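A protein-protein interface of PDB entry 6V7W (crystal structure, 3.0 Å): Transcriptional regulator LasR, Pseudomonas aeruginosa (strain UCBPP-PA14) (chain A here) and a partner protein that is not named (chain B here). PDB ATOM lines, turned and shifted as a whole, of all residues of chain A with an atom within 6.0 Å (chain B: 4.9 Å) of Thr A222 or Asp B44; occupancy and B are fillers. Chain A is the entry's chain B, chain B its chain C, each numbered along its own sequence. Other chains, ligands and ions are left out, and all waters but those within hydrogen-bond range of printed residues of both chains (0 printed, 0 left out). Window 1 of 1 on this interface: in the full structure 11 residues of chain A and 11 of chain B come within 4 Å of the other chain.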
ATOM      1  N   GLU A  11      15.965  17.317  36.652  1.00  0.00           N
ATOM      2  CA  GLU A  11      16.732  17.014  35.451  1.00  0.00           C
ATOM      3  C   GLU A  11      18.176  16.703  35.828  1.00  0.00           C
ATOM      4  O   GLU A  11      18.927  17.592  36.235  1.00  0.00           O
ATOM      5  CB  GLU A  11      16.665  18.189  34.478  1.00  0.00           C
ATOM      6  CG  GLU A  11      16.803  19.552  35.150  1.00  0.00           C
ATOM      7  CD  GLU A  11      16.329  20.694  34.277  1.00  0.00           C
ATOM      8  OE1 GLU A  11      16.436  20.583  33.037  1.00  0.00           O
ATOM      9  OE2 GLU A  11      15.841  21.700  34.833  1.00  0.00           O
ATOM     10  N   GLU A  18      26.817  20.212  32.432  1.00  0.00           N
ATOM     11  CA  GLU A  18      25.380  20.445  32.504  1.00  0.00           C
ATOM     12  C   GLU A  18      24.869  20.241  33.922  1.00  0.00           C
ATOM     13  O   GLU A  18      24.113  21.069  34.442  1.00  0.00           O
ATOM     14  CB  GLU A  18      24.639  19.531  31.529  1.00  0.00           C
ATOM     15  CG  GLU A  18      23.126  19.654  31.632  1.00  0.00           C
ATOM     16  CD  GLU A  18      22.391  18.895  30.544  1.00  0.00           C
ATOM     17  OE1 GLU A  18      23.058  18.215  29.736  1.00  0.00           O
ATOM     18  OE2 GLU A  18      21.144  18.968  30.507  1.00  0.00           O
ATOM     19  N   ASN A 209      13.065  30.131  18.713  1.00  0.00           N
ATOM     20  CA  ASN A 209      12.794  28.805  19.255  1.00  0.00           C
ATOM     21  C   ASN A 209      13.477  27.723  18.433  1.00  0.00           C
ATOM     22  O   ASN A 209      13.923  26.709  18.985  1.00  0.00           O
ATOM     23  CB  ASN A 209      11.288  28.557  19.304  1.00  0.00           C
ATOM     24  CG  ASN A 209      10.684  28.896  20.645  1.00  0.00           C
ATOM     25  OD1 ASN A 209      11.299  29.578  21.460  1.00  0.00           O
ATOM     26  ND2 ASN A 209       9.466  28.420  20.881  1.00  0.00           N
ATOM     27  N   MET A 212      17.287  27.891  19.476  1.00  0.00           N
ATOM     28  CA  MET A 212      17.560  27.311  20.788  1.00  0.00           C
ATOM     29  C   MET A 212      17.519  25.791  20.744  1.00  0.00           C
ATOM     30  O   MET A 212      18.280  25.129  21.458  1.00  0.00           O
ATOM     31  CB  MET A 212      16.561  27.830  21.826  1.00  0.00           C
ATOM     32  CG  MET A 212      16.511  29.346  21.980  1.00  0.00           C
ATOM     33  SD  MET A 212      17.962  30.113  22.740  1.00  0.00           S
ATOM     34  CE  MET A 212      18.540  28.826  23.837  1.00  0.00           C
ATOM     35  N   ARG A 216      20.541  23.535  21.981  1.00  0.00           N
ATOM     36  CA  ARG A 216      20.391  22.527  23.024  1.00  0.00           C
ATOM     37  C   ARG A 216      20.887  21.158  22.570  1.00  0.00           C
ATOM     38  O   ARG A 216      21.353  20.366  23.399  1.00  0.00           O
ATOM     39  CB  ARG A 216      18.931  22.469  23.479  1.00  0.00           C
ATOM     40  CG  ARG A 216      18.554  23.639  24.384  1.00  0.00           C
ATOM     41  CD  ARG A 216      17.055  23.884  24.489  1.00  0.00           C
ATOM     42  NE  ARG A 216      16.246  22.727  24.122  1.00  0.00           N
ATOM     43  CZ  ARG A 216      15.234  22.772  23.263  1.00  0.00           C
ATOM     44  NH1 ARG A 216      14.899  23.920  22.687  1.00  0.00           N
ATOM     45  NH2 ARG A 216      14.549  21.671  22.986  1.00  0.00           N
ATOM     46  N   GLY A 220      23.982  19.059  24.201  1.00  0.00           N
ATOM     47  CA  GLY A 220      23.526  17.807  24.770  1.00  0.00           C
ATOM     48  C   GLY A 220      22.599  17.970  25.950  1.00  0.00           C
ATOM     49  O   GLY A 220      22.546  17.090  26.814  1.00  0.00           O
ATOM     50  N   VAL A 221      21.861  19.077  26.009  1.00  0.00           N
ATOM     51  CA  VAL A 221      21.015  19.390  27.155  1.00  0.00           C
ATOM     52  C   VAL A 221      19.549  19.279  26.759  1.00  0.00           C
ATOM     53  O   VAL A 221      19.225  19.023  25.595  1.00  0.00           O
ATOM     54  CB  VAL A 221      21.332  20.793  27.701  1.00  0.00           C
ATOM     55  CG1 VAL A 221      22.830  20.983  27.825  1.00  0.00           C
ATOM     56  CG2 VAL A 221      20.741  21.856  26.792  1.00  0.00           C
ATOM     57  N   THR A 222      18.651  19.479  27.730  1.00  0.00           N
ATOM     58  CA  THR A 222      17.215  19.401  27.487  1.00  0.00           C
ATOM     59  C   THR A 222      16.491  20.660  27.952  1.00  0.00           C
ATOM     60  O   THR A 222      15.278  20.621  28.184  1.00  0.00           O
ATOM     61  CB  THR A 222      16.614  18.170  28.171  1.00  0.00           C
ATOM     62  OG1 THR A 222      16.868  18.233  29.580  1.00  0.00           O
ATOM     63  CG2 THR A 222      17.216  16.893  27.607  1.00  0.00           C
ATOM     64  N   SER A 223      17.206  21.772  28.092  1.00  0.00           N
ATOM     65  CA  SER A 223      16.604  23.029  28.513  1.00  0.00           C
ATOM     66  C   SER A 223      17.521  24.165  28.089  1.00  0.00           C
ATOM     67  O   SER A 223      18.746  24.028  28.097  1.00  0.00           O
ATOM     68  CB  SER A 223      16.360  23.072  30.025  1.00  0.00           C
ATOM     69  OG  SER A 223      17.379  23.804  30.682  1.00  0.00           O
ATOM     70  N   ARG A 224      16.910  25.291  27.724  1.00  0.00           N
ATOM     71  CA  ARG A 224      17.676  26.406  27.182  1.00  0.00           C
ATOM     72  C   ARG A 224      18.452  27.150  28.263  1.00  0.00           C
ATOM     73  O   ARG A 224      19.605  27.538  28.043  1.00  0.00           O
ATOM     74  CB  ARG A 224      16.747  27.364  26.439  1.00  0.00           C
ATOM     75  CG  ARG A 224      15.497  27.768  27.198  1.00  0.00           C
ATOM     76  CD  ARG A 224      14.697  28.749  26.368  1.00  0.00           C
ATOM     77  NE  ARG A 224      14.379  28.182  25.062  1.00  0.00           N
ATOM     78  CZ  ARG A 224      13.435  28.648  24.253  1.00  0.00           C
ATOM     79  NH1 ARG A 224      12.715  29.702  24.610  1.00  0.00           N
ATOM     80  NH2 ARG A 224      13.216  28.062  23.086  1.00  0.00           N
ATOM     81  N   ARG A 225      17.836  27.364  29.430  1.00  0.00           N
ATOM     82  CA  ARG A 225      18.504  28.103  30.496  1.00  0.00           C
ATOM     83  C   ARG A 225      19.763  27.384  30.967  1.00  0.00           C
ATOM     84  O   ARG A 225      20.769  28.027  31.289  1.00  0.00           O
ATOM     85  CB  ARG A 225      17.534  28.326  31.658  1.00  0.00           C
ATOM     86  CG  ARG A 225      16.208  28.936  31.224  1.00  0.00           C
ATOM     87  CD  ARG A 225      15.610  29.849  32.286  1.00  0.00           C
ATOM     88  NE  ARG A 225      15.147  29.112  33.459  1.00  0.00           N
ATOM     89  CZ  ARG A 225      15.804  29.054  34.611  1.00  0.00           C
ATOM     90  NH1 ARG A 225      16.960  29.689  34.752  1.00  0.00           N
ATOM     91  NH2 ARG A 225      15.305  28.361  35.626  1.00  0.00           N
ATOM     92  N   ARG B  40       7.890  26.143  29.451  1.00  0.00           N
ATOM     93  CA  ARG B  40       8.987  26.235  28.494  1.00  0.00           C
ATOM     94  C   ARG B  40       9.927  25.041  28.614  1.00  0.00           C
ATOM     95  O   ARG B  40      10.310  24.436  27.607  1.00  0.00           O
ATOM     96  CB  ARG B  40       9.743  27.546  28.706  1.00  0.00           C
ATOM     97  CG  ARG B  40      10.976  27.716  27.845  1.00  0.00           C
ATOM     98  CD  ARG B  40      10.599  28.151  26.440  1.00  0.00           C
ATOM     99  NE  ARG B  40      10.410  27.018  25.538  1.00  0.00           N
ATOM    100  CZ  ARG B  40       9.883  27.111  24.322  1.00  0.00           C
ATOM    101  NH1 ARG B  40       9.755  26.028  23.567  1.00  0.00           N
ATOM    102  NH2 ARG B  40       9.483  28.288  23.860  1.00  0.00           N
ATOM    103  N   ASP B  41      10.321  24.695  29.843  1.00  0.00           N
ATOM    104  CA  ASP B  41      11.221  23.561  30.034  1.00  0.00           C
ATOM    105  C   ASP B  41      10.574  22.260  29.576  1.00  0.00           C
ATOM    106  O   ASP B  41      11.249  21.382  29.025  1.00  0.00           O
ATOM    107  CB  ASP B  41      11.647  23.466  31.499  1.00  0.00           C
ATOM    108  CG  ASP B  41      12.544  24.612  31.920  1.00  0.00           C
ATOM    109  OD1 ASP B  41      13.174  25.232  31.036  1.00  0.00           O
ATOM    110  OD2 ASP B  41      12.624  24.893  33.133  1.00  0.00           O
ATOM    111  N   ALA B  42       9.267  22.113  29.806  1.00  0.00           N
ATOM    112  CA  ALA B  42       8.558  20.932  29.325  1.00  0.00           C
ATOM    113  C   ALA B  42       8.574  20.856  27.803  1.00  0.00           C
ATOM    114  O   ALA B  42       8.796  19.784  27.231  1.00  0.00           O
ATOM    115  CB  ALA B  42       7.121  20.932  29.848  1.00  0.00           C
ATOM    116  N   LEU B  43       8.345  21.987  27.131  1.00  0.00           N
ATOM    117  CA  LEU B  43       8.424  22.007  25.673  1.00  0.00           C
ATOM    118  C   LEU B  43       9.857  21.814  25.193  1.00  0.00           C
ATOM    119  O   LEU B  43      10.096  21.088  24.221  1.00  0.00           O
ATOM    120  CB  LEU B  43       7.844  23.313  25.130  1.00  0.00           C
ATOM    121  CG  LEU B  43       7.558  23.338  23.627  1.00  0.00           C
ATOM    122  CD1 LEU B  43       6.757  22.115  23.211  1.00  0.00           C
ATOM    123  CD2 LEU B  43       6.824  24.612  23.242  1.00  0.00           C
ATOM    124  N   ASP B  44      10.822  22.454  25.857  1.00  0.00           N
ATOM    125  CA  ASP B  44      12.217  22.307  25.452  1.00  0.00           C
ATOM    126  C   ASP B  44      12.675  20.862  25.594  1.00  0.00           C
ATOM    127  O   ASP B  44      13.404  20.347  24.738  1.00  0.00           O
ATOM    128  CB  ASP B  44      13.105  23.241  26.273  1.00  0.00           C
ATOM    129  CG  ASP B  44      13.180  24.635  25.686  1.00  0.00           C
ATOM    130  OD1 ASP B  44      14.295  25.193  25.609  1.00  0.00           O
ATOM    131  OD2 ASP B  44      12.123  25.172  25.292  1.00  0.00           O
ATOM    132  N   TRP B  45      12.262  20.192  26.672  1.00  0.00           N
ATOM    133  CA  TRP B  45      12.614  18.786  26.840  1.00  0.00           C
ATOM    134  C   TRP B  45      11.951  17.929  25.770  1.00  0.00           C
ATOM    135  O   TRP B  45      12.571  17.000  25.239  1.00  0.00           O
ATOM    136  CB  TRP B  45      12.214  18.303  28.234  1.00  0.00           C
ATOM    137  CG  TRP B  45      12.796  16.969  28.599  1.00  0.00           C
ATOM    138  CD1 TRP B  45      13.729  16.261  27.899  1.00  0.00           C
ATOM    139  CD2 TRP B  45      12.456  16.167  29.736  1.00  0.00           C
ATOM    140  NE1 TRP B  45      14.005  15.078  28.538  1.00  0.00           N
ATOM    141  CE2 TRP B  45      13.235  14.995  29.668  1.00  0.00           C
ATOM    142  CE3 TRP B  45      11.575  16.330  30.809  1.00  0.00           C
ATOM    143  CZ2 TRP B  45      13.158  13.992  30.628  1.00  0.00           C
ATOM    144  CZ3 TRP B  45      11.503  15.335  31.762  1.00  0.00           C
ATOM    145  CH2 TRP B  45      12.289  14.180  31.666  1.00  0.00           C
ATOM    146  N   LEU B  46      10.692  18.227  25.439  1.00  0.00           N
ATOM    147  CA  LEU B  46       9.988  17.437  24.435  1.00  0.00           C
ATOM    148  C   LEU B  46      10.649  17.573  23.071  1.00  0.00           C
ATOM    149  O   LEU B  46      10.836  16.579  22.361  1.00  0.00           O
ATOM    150  CB  LEU B  46       8.522  17.861  24.361  1.00  0.00           C
ATOM    151  CG  LEU B  46       7.627  16.952  23.518  1.00  0.00           C
ATOM    152  CD1 LEU B  46       7.589  15.550  24.106  1.00  0.00           C
ATOM    153  CD2 LEU B  46       6.225  17.529  23.391  1.00  0.00           C
ATOM    154  N   GLU B  47      11.013  18.800  22.689  1.00  0.00           N
ATOM    155  CA  GLU B  47      11.680  19.003  21.409  1.00  0.00           C
ATOM    156  C   GLU B  47      13.068  18.377  21.405  1.00  0.00           C
ATOM    157  O   GLU B  47      13.446  17.704  20.438  1.00  0.00           O
ATOM    158  CB  GLU B  47      11.766  20.496  21.090  1.00  0.00           C
ATOM    159  CG  GLU B  47      10.430  21.220  21.107  1.00  0.00           C
ATOM    160  CD  GLU B  47      10.587  22.726  21.058  1.00  0.00           C
ATOM    161  OE1 GLU B  47      11.739  23.208  21.121  1.00  0.00           O
ATOM    162  OE2 GLU B  47       9.560  23.431  20.959  1.00  0.00           O
ATOM    163  N   SER B  48      13.839  18.579  22.477  1.00  0.00           N
ATOM    164  CA  SER B  48      15.197  18.045  22.520  1.00  0.00           C
ATOM    165  C   SER B  48      15.204  16.522  22.548  1.00  0.00           C
ATOM    166  O   SER B  48      16.046  15.890  21.901  1.00  0.00           O
ATOM    167  CB  SER B  48      15.944  18.601  23.731  1.00  0.00           C
ATOM    168  OG  SER B  48      16.270  19.966  23.546  1.00  0.00           O
ATOM    169  N   ALA B  49      14.277  15.915  23.294  1.00  0.00           N
ATOM    170  CA  ALA B  49      14.235  14.457  23.356  1.00  0.00           C
ATOM    171  C   ALA B  49      13.785  13.858  22.029  1.00  0.00           C
ATOM    172  O   ALA B  49      14.386  12.891  21.546  1.00  0.00           O
ATOM    173  CB  ALA B  49      13.319  14.001  24.491  1.00  0.00           C
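O of Asp B44 lies within hydrogen-bond range of OG of Ser B48, at 3.1 Å.
OD2 of Asp B44 lies within salt-bridge range of NE of Arg B40, at 2.5 Å.
OD1 of Asn A209 is in hydrogen-bond range of NH2 of Arg A224 (2.9 Å).
O of Arg A216 lies within hydrogen-bond range of N of Val A221 (3.0 Å).
The guanidinium group (NH1) of Arg B40 lies within salt-bridge range of the side-chain carboxylate (OE2) of Glu B47, at 3.7 Å.
Ser B48 touches Val A221 (OG to O, 3.7 Å).
Asp B44 touches Thr A222 (C to O, 3.7 Å).
Ser A223 touches Asp B41 (CB to OD1, 3.98 Å).
Arg A224 touches Arg B40 (NH1 to CD, 3.2 Å).
The side-chain hydroxyl (OG) of Ser B48 is in hydrogen-bond range of the guanidinium group (NH2) of Arg A216 (2.5 Å).
OE1 of Glu B47 is in salt-bridge range of NH1 of Arg A216, 3.6 Å away.
NH1 of Arg A216 is in salt-bridge range of OD1 of Asp B44 (3.2 Å).
The side-chain carboxylate of Asp B44 lies within salt-bridge range of the guanidinium group of Arg A224 (3.0 Å).
O of Thr A222 lies within hydrogen-bond range of N of Trp B45, 3.4 Å away.
The side-chain amide nitrogen (ND2) of Asn A209 sits close to the guanidinium group (NH2) of Arg B40 (3.0 Å).
Glu A18 touches none of the printed residues of chain B.
Of the printed residues of chain B, Val A221 touches Ser B48 (3.7 Å).
Of chain B, only Asp B44 and Trp B45 come within 4 Å of Thr A222.
Arg A225 touches none of the printed residues of chain B.
Printed residues of chain A within 4 Å of Asp B44: Arg A216 (2.5 Å), Thr A222 (3.7 Å) and Arg A224 (3.0 Å).
Printed residues of chain A within 4 Å of Glu B47: Arg A216.
Of the 11 printed residues of chain A, 6 touch a printed residue of chain B.
Along chain A the printed residues that touch a printed residue of chain B span positions 209 to 224.
Of the 10 printed residues of chain B, 6 touch a printed residue of chain A.
Printed residues of chain B that touch a printed residue of chain A: Arg B40, Asp B41, Asp B44, Trp B45, Glu B47 and Ser B48.
Among the printed residues, 10 pairs touch across the chains.
Among the printed residues, Asp or Glu carboxylates within 4 Å of a Lys or Arg side-chain nitrogen of the other chain: Arg A216 with Asp B44, Arg A216 with Glu B47 and Arg A224 with Asp B44.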
